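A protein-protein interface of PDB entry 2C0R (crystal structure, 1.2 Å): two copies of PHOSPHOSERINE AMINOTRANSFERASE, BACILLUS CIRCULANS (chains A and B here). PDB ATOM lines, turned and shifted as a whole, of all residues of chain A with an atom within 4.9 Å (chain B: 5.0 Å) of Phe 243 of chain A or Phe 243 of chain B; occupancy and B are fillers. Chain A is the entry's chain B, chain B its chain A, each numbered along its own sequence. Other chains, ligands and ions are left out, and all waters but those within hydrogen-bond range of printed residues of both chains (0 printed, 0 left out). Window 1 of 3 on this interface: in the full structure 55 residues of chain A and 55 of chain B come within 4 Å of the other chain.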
ATOM      1  N   ALA A  23     -13.744  11.616 -28.866  1.00  0.00           N
ATOM      2  CA  ALA A  23     -13.410  11.572 -27.425  1.00  0.00           C
ATOM      3  C   ALA A  23     -14.674  11.826 -26.629  1.00  0.00           C
ATOM      4  O   ALA A  23     -14.940  11.210 -25.582  1.00  0.00           O
ATOM      5  CB  ALA A  23     -12.309  12.553 -27.094  1.00  0.00           C
ATOM      6  N   PHE A  27     -16.368   9.446 -23.653  1.00  0.00           N
ATOM      7  CA  PHE A  27     -15.865  10.119 -22.476  1.00  0.00           C
ATOM      8  C   PHE A  27     -16.336   9.512 -21.167  1.00  0.00           C
ATOM      9  O   PHE A  27     -15.600   9.411 -20.170  1.00  0.00           O
ATOM     10  CB  PHE A  27     -16.255  11.603 -22.510  1.00  0.00           C
ATOM     11  CG  PHE A  27     -15.538  12.415 -21.443  1.00  0.00           C
ATOM     12  CD1 PHE A  27     -14.242  12.840 -21.601  1.00  0.00           C
ATOM     13  CD2 PHE A  27     -16.173  12.779 -20.261  1.00  0.00           C
ATOM     14  CE1 PHE A  27     -13.562  13.599 -20.670  1.00  0.00           C
ATOM     15  CE2 PHE A  27     -15.507  13.525 -19.294  1.00  0.00           C
ATOM     16  CZ  PHE A  27     -14.208  13.932 -19.487  1.00  0.00           C
ATOM     17  N   ILE A  37     -11.786   6.637 -19.781  1.00  0.00           N
ATOM     18  CA  ILE A  37     -10.317   6.447 -19.845  1.00  0.00           C
ATOM     19  C   ILE A  37      -9.644   7.210 -18.704  1.00  0.00           C
ATOM     20  O   ILE A  37      -8.603   6.759 -18.186  1.00  0.00           O
ATOM     21  CB  ILE A  37      -9.811   6.826 -21.240  1.00  0.00           C
ATOM     22  CG1 ILE A  37      -8.384   6.265 -21.473  1.00  0.00           C
ATOM     23  CG2 ILE A  37      -9.826   8.316 -21.469  1.00  0.00           C
ATOM     24  CD1 ILE A  37      -8.336   4.746 -21.534  1.00  0.00           C
ATOM     25  N   MET A  38     -10.213   8.302 -18.221  1.00  0.00           N
ATOM     26  CA  MET A  38      -9.707   9.087 -17.111  1.00  0.00           C
ATOM     27  C   MET A  38      -9.764   8.430 -15.735  1.00  0.00           C
ATOM     28  O   MET A  38      -9.102   8.861 -14.799  1.00  0.00           O
ATOM     29  CB  MET A  38     -10.540  10.359 -16.904  1.00  0.00           C
ATOM     30  CG  MET A  38     -10.338  11.426 -17.952  1.00  0.00           C
ATOM     31  SD  MET A  38     -11.203  12.883 -17.364  1.00  0.00           S
ATOM     32  CE  MET A  38     -10.179  13.515 -16.050  1.00  0.00           C
ATOM     33  N   PRO A 241       0.188  11.784 -17.864  1.00  0.00           N
ATOM     34  CA  PRO A 241      -0.979  12.569 -18.221  1.00  0.00           C
ATOM     35  C   PRO A 241      -1.865  11.723 -19.132  1.00  0.00           C
ATOM     36  O   PRO A 241      -1.851  11.877 -20.344  1.00  0.00           O
ATOM     37  CB  PRO A 241      -0.401  13.760 -18.978  1.00  0.00           C
ATOM     38  CG  PRO A 241       0.856  13.217 -19.578  1.00  0.00           C
ATOM     39  CD  PRO A 241       1.393  12.252 -18.537  1.00  0.00           C
ATOM     40  N   SER A 242      -2.618  10.818 -18.496  1.00  0.00           N
ATOM     41  CA  SER A 242      -3.211   9.716 -19.257  1.00  0.00           C
ATOM     42  C   SER A 242      -4.270  10.222 -20.236  1.00  0.00           C
ATOM     43  O   SER A 242      -4.318   9.758 -21.369  1.00  0.00           O
ATOM     44  CB  SER A 242      -3.740   8.637 -18.301  1.00  0.00           C
ATOM     45  OG  SER A 242      -4.693   9.154 -17.401  1.00  0.00           O
ATOM     46  N   PHE A 243      -5.103  11.188 -19.816  1.00  0.00           N
ATOM     47  CA  PHE A 243      -6.119  11.676 -20.778  1.00  0.00           C
ATOM     48  C   PHE A 243      -5.449  12.404 -21.924  1.00  0.00           C
ATOM     49  O   PHE A 243      -5.878  12.297 -23.073  1.00  0.00           O
ATOM     50  CB  PHE A 243      -7.146  12.563 -20.071  1.00  0.00           C
ATOM     51  CG  PHE A 243      -8.331  12.814 -21.000  1.00  0.00           C
ATOM     52  CD1 PHE A 243      -9.162  11.746 -21.303  1.00  0.00           C
ATOM     53  CD2 PHE A 243      -8.549  14.074 -21.512  1.00  0.00           C
ATOM     54  CE1 PHE A 243     -10.253  11.949 -22.146  1.00  0.00           C
ATOM     55  CE2 PHE A 243      -9.623  14.292 -22.348  1.00  0.00           C
ATOM     56  CZ  PHE A 243     -10.461  13.224 -22.645  1.00  0.00           C
ATOM     57  N   GLY A 244      -4.366  13.127 -21.647  1.00  0.00           N
ATOM     58  CA  GLY A 244      -3.671  13.895 -22.667  1.00  0.00           C
ATOM     59  C   GLY A 244      -3.053  12.931 -23.670  1.00  0.00           C
ATOM     60  O   GLY A 244      -3.063  13.155 -24.880  1.00  0.00           O
ATOM     61  N   ILE A 245      -2.511  11.820 -23.186  1.00  0.00           N
ATOM     62  CA  ILE A 245      -1.898  10.836 -24.091  1.00  0.00           C
ATOM     63  C   ILE A 245      -2.961  10.126 -24.910  1.00  0.00           C
ATOM     64  O   ILE A 245      -2.765   9.879 -26.114  1.00  0.00           O
ATOM     65  CB  ILE A 245      -1.020   9.868 -23.263  1.00  0.00           C
ATOM     66  CG1 ILE A 245       0.168  10.629 -22.712  1.00  0.00           C
ATOM     67  CG2 ILE A 245      -0.613   8.671 -24.121  1.00  0.00           C
ATOM     68  CD1 ILE A 245       0.829   9.881 -21.562  1.00  0.00           C
ATOM     69  N   TYR A 246      -4.098   9.851 -24.255  1.00  0.00           N
ATOM     70  CA  TYR A 246      -5.237   9.295 -25.008  1.00  0.00           C
ATOM     71  C   TYR A 246      -5.621  10.223 -26.151  1.00  0.00           C
ATOM     72  O   TYR A 246      -5.886   9.801 -27.271  1.00  0.00           O
ATOM     73  CB  TYR A 246      -6.353   9.047 -23.979  1.00  0.00           C
ATOM     74  CG  TYR A 246      -7.713   8.987 -24.649  1.00  0.00           C
ATOM     75  CD1 TYR A 246      -8.209   7.820 -25.225  1.00  0.00           C
ATOM     76  CD2 TYR A 246      -8.531  10.126 -24.702  1.00  0.00           C
ATOM     77  CE1 TYR A 246      -9.465   7.840 -25.838  1.00  0.00           C
ATOM     78  CE2 TYR A 246      -9.765  10.172 -25.303  1.00  0.00           C
ATOM     79  CZ  TYR A 246     -10.213   8.978 -25.866  1.00  0.00           C
ATOM     80  OH  TYR A 246     -11.448   9.013 -26.436  1.00  0.00           O
ATOM     81  N   MET A 247      -5.671  11.535 -25.844  1.00  0.00           N
ATOM     82  CA  MET A 247      -6.033  12.500 -26.889  1.00  0.00           C
ATOM     83  C   MET A 247      -4.962  12.595 -27.973  1.00  0.00           C
ATOM     84  O   MET A 247      -5.262  12.732 -29.143  1.00  0.00           O
ATOM     85  CB  MET A 247      -6.252  13.880 -26.250  1.00  0.00           C
ATOM     86  CG  MET A 247      -7.518  14.058 -25.428  1.00  0.00           C
ATOM     87  SD  MET A 247      -9.034  13.712 -26.285  1.00  0.00           S
ATOM     88  CE  MET A 247      -9.165  15.142 -27.357  1.00  0.00           C
ATOM     89  N   ALA B  23     -18.909  17.209 -18.180  1.00  0.00           N
ATOM     90  CA  ALA B  23     -17.752  17.477 -19.024  1.00  0.00           C
ATOM     91  C   ALA B  23     -18.011  16.906 -20.435  1.00  0.00           C
ATOM     92  O   ALA B  23     -17.650  17.547 -21.440  1.00  0.00           O
ATOM     93  CB  ALA B  23     -16.486  16.945 -18.423  1.00  0.00           C
ATOM     94  N   PHE B  27     -17.918  19.052 -24.039  1.00  0.00           N
ATOM     95  CA  PHE B  27     -16.560  18.705 -24.459  1.00  0.00           C
ATOM     96  C   PHE B  27     -16.223  19.303 -25.815  1.00  0.00           C
ATOM     97  O   PHE B  27     -15.068  19.705 -26.001  1.00  0.00           O
ATOM     98  CB  PHE B  27     -16.459  17.186 -24.559  1.00  0.00           C
ATOM     99  CG  PHE B  27     -15.061  16.641 -24.731  1.00  0.00           C
ATOM    100  CD1 PHE B  27     -14.281  16.331 -23.630  1.00  0.00           C
ATOM    101  CD2 PHE B  27     -14.516  16.401 -25.977  1.00  0.00           C
ATOM    102  CE1 PHE B  27     -13.011  15.807 -23.723  1.00  0.00           C
ATOM    103  CE2 PHE B  27     -13.252  15.871 -26.115  1.00  0.00           C
ATOM    104  CZ  PHE B  27     -12.494  15.531 -24.987  1.00  0.00           C
ATOM    105  N   ILE B  37     -13.020  23.695 -24.272  1.00  0.00           N
ATOM    106  CA  ILE B  37     -12.088  24.338 -23.327  1.00  0.00           C
ATOM    107  C   ILE B  37     -10.643  23.998 -23.613  1.00  0.00           C
ATOM    108  O   ILE B  37      -9.739  24.820 -23.361  1.00  0.00           O
ATOM    109  CB  ILE B  37     -12.428  23.944 -21.872  1.00  0.00           C
ATOM    110  CG1 ILE B  37     -11.723  24.849 -20.841  1.00  0.00           C
ATOM    111  CG2 ILE B  37     -12.120  22.489 -21.601  1.00  0.00           C
ATOM    112  CD1 ILE B  37     -12.289  26.249 -20.891  1.00  0.00           C
ATOM    113  N   MET B  38     -10.407  22.818 -24.189  1.00  0.00           N
ATOM    114  CA  MET B  38      -9.050  22.425 -24.573  1.00  0.00           C
ATOM    115  C   MET B  38      -8.412  23.222 -25.691  1.00  0.00           C
ATOM    116  O   MET B  38      -7.203  23.094 -25.905  1.00  0.00           O
ATOM    117  CB  MET B  38      -9.057  20.989 -25.112  1.00  0.00           C
ATOM    118  CG  MET B  38      -9.211  19.920 -24.045  1.00  0.00           C
ATOM    119  SD  MET B  38      -9.165  18.402 -25.046  1.00  0.00           S
ATOM    120  CE  MET B  38      -8.592  17.268 -23.777  1.00  0.00           C
ATOM    121  N   PRO B 241      -1.902  22.627 -17.623  1.00  0.00           N
ATOM    122  CA  PRO B 241      -2.748  21.473 -17.984  1.00  0.00           C
ATOM    123  C   PRO B 241      -4.224  21.871 -17.947  1.00  0.00           C
ATOM    124  O   PRO B 241      -4.933  21.589 -16.981  1.00  0.00           O
ATOM    125  CB  PRO B 241      -2.361  20.435 -16.927  1.00  0.00           C
ATOM    126  CG  PRO B 241      -1.974  21.257 -15.736  1.00  0.00           C
ATOM    127  CD  PRO B 241      -1.292  22.502 -16.273  1.00  0.00           C
ATOM    128  N   SER B 242      -4.612  22.558 -19.014  1.00  0.00           N
ATOM    129  CA  SER B 242      -5.851  23.329 -18.923  1.00  0.00           C
ATOM    130  C   SER B 242      -7.056  22.398 -18.799  1.00  0.00           C
ATOM    131  O   SER B 242      -7.957  22.716 -18.025  1.00  0.00           O
ATOM    132  CB  SER B 242      -5.983  24.322 -20.071  1.00  0.00           C
ATOM    133  OG  SER B 242      -5.672  23.714 -21.274  1.00  0.00           O
ATOM    134  N   PHE B 243      -7.107  21.274 -19.474  1.00  0.00           N
ATOM    135  CA  PHE B 243      -8.285  20.389 -19.328  1.00  0.00           C
ATOM    136  C   PHE B 243      -8.300  19.790 -17.934  1.00  0.00           C
ATOM    137  O   PHE B 243      -9.358  19.654 -17.346  1.00  0.00           O
ATOM    138  CB  PHE B 243      -8.330  19.299 -20.394  1.00  0.00           C
ATOM    139  CG  PHE B 243      -9.631  18.525 -20.378  1.00  0.00           C
ATOM    140  CD1 PHE B 243     -10.798  19.134 -20.823  1.00  0.00           C
ATOM    141  CD2 PHE B 243      -9.686  17.216 -19.936  1.00  0.00           C
ATOM    142  CE1 PHE B 243     -12.007  18.535 -20.869  1.00  0.00           C
ATOM    143  CE2 PHE B 243     -10.943  16.626 -19.951  1.00  0.00           C
ATOM    144  CZ  PHE B 243     -12.091  17.256 -20.357  1.00  0.00           C
ATOM    145  N   GLY B 244      -7.118  19.441 -17.421  1.00  0.00           N
ATOM    146  CA  GLY B 244      -7.093  18.904 -16.060  1.00  0.00           C
ATOM    147  C   GLY B 244      -7.601  19.916 -15.049  1.00  0.00           C
ATOM    148  O   GLY B 244      -8.295  19.568 -14.092  1.00  0.00           O
ATOM    149  N   ILE B 245      -7.201  21.200 -15.195  1.00  0.00           N
ATOM    150  CA  ILE B 245      -7.633  22.196 -14.259  1.00  0.00           C
ATOM    151  C   ILE B 245      -9.126  22.470 -14.383  1.00  0.00           C
ATOM    152  O   ILE B 245      -9.800  22.631 -13.377  1.00  0.00           O
ATOM    153  CB  ILE B 245      -6.801  23.477 -14.430  1.00  0.00           C
ATOM    154  CG1 ILE B 245      -5.361  23.177 -13.985  1.00  0.00           C
ATOM    155  CG2 ILE B 245      -7.375  24.650 -13.683  1.00  0.00           C
ATOM    156  CD1 ILE B 245      -4.351  24.201 -14.506  1.00  0.00           C
ATOM    157  N   TYR B 246      -9.652  22.494 -15.619  1.00  0.00           N
ATOM    158  CA  TYR B 246     -11.077  22.559 -15.835  1.00  0.00           C
ATOM    159  C   TYR B 246     -11.805  21.419 -15.111  1.00  0.00           C
ATOM    160  O   TYR B 246     -12.860  21.615 -14.487  1.00  0.00           O
ATOM    161  CB  TYR B 246     -11.342  22.507 -17.351  1.00  0.00           C
ATOM    162  CG  TYR B 246     -12.733  22.043 -17.708  1.00  0.00           C
ATOM    163  CD1 TYR B 246     -13.836  22.907 -17.681  1.00  0.00           C
ATOM    164  CD2 TYR B 246     -12.952  20.722 -18.104  1.00  0.00           C
ATOM    165  CE1 TYR B 246     -15.078  22.462 -18.012  1.00  0.00           C
ATOM    166  CE2 TYR B 246     -14.201  20.265 -18.432  1.00  0.00           C
ATOM    167  CZ  TYR B 246     -15.259  21.147 -18.382  1.00  0.00           C
ATOM    168  OH  TYR B 246     -16.490  20.663 -18.726  1.00  0.00           O
ATOM    169  N   MET B 247     -11.246  20.217 -15.171  1.00  0.00           N
ATOM    170  CA  MET B 247     -11.902  19.068 -14.518  1.00  0.00           C
ATOM    171  C   MET B 247     -11.771  19.145 -13.009  1.00  0.00           C
ATOM    172  O   MET B 247     -12.738  18.816 -12.299  1.00  0.00           O
ATOM    173  CB  MET B 247     -11.276  17.768 -14.989  1.00  0.00           C
ATOM    174  CG  MET B 247     -11.570  17.272 -16.387  1.00  0.00           C
ATOM    175  SD  MET B 247     -13.339  17.044 -16.721  1.00  0.00           S
ATOM    176  CE  MET B 247     -13.677  15.503 -15.869  1.00  0.00           C
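Among the printed residues, merely in contact across the chains: Ala 23 of chain A with Phe 27 of chain B (3.6 Å), Phe 27 of chain A with Ala 23 of chain B (3.7 Å), Phe 27 of chain A with Phe 27 of chain B (3.8 Å), Phe 27 of chain A with Phe 243 of chain B (3.95 Å), Phe 27 of chain A with Met 247 of chain B (3.98 Å), Met 38 of chain A with Met 247 of chain B (3.9 Å), Phe 243 of chain A with Phe 27 of chain B (3.8 Å), Phe 243 of chain A with Met 38 of chain B (3.5 Å), Phe 243 of chain A with Phe 243 of chain B (3.6 Å) and Met 247 of chain A with Met 38 of chain B (3.8 Å).
Phe 243 of chain A touches three residues of chain B.
Of chain A, only Phe 27 (3.95 Å) and Phe 243 (3.6 Å) come within 4 Å of Phe 243 of chain B.
Of the printed residues of chain A, Met 247 of chain B touches Phe 27 (3.98 Å) and Met 38 (3.9 Å).
Of the printed residues of chain B, Ala 23 of chain A touches Phe 27 (3.6 Å).
Printed residues of chain A within 4 Å of Ala 23 of chain B: Phe 27 (3.7 Å).
Of the printed residues of chain A, Phe 27 of chain B touches Ala 23 (3.6 Å), Phe 27 (3.8 Å) and Phe 243 (3.8 Å).
Gly 244 of chain A touches none of the printed residues of chain B.
The nearest printed residue of chain B that does not touch Ala 23 of chain A is Met 38 of chain B (6.9 Å).
Of the 11 printed residues of chain B, 5 touch a printed residue of chain A.
Printed residues of chain B that touch a printed residue of chain A: Ala 23, Phe 27, Met 38, Phe 243 and Met 247.
Printed residues of chain A that touch a printed residue of chain B: Ala 23, Phe 27, Met 38, Phe 243 and Met 247.
Among the printed residues, 10 pairs touch across the chains.
Among the printed residues, no Asp or Glu carboxylate lies within 4 Å of a Lys or Arg side-chain nitrogen of the other chain.
Ala 23 of chain A touches Phe 27 of chain B, and with the chains exchanged Phe 27 of chain A touches Ala 23 of chain B.
Phe 27 of chain B touches its own counterpart, Phe 27 of chain A.
Met 38 of chain A touches Met 247 of chain B, and with the chains exchanged Met 247 of chain A touches Met 38 of chain B.
Phe 243 of chain A touches Met 38 of chain B, but with the chains exchanged Met 38 of chain A does not touch Phe 243 of chain B (4.6 Å).
11 positions are printed for both chains.
Of the 10 pairs that touch across the chains among the printed residues, 8 have their exchanged pair printed and touching as well.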
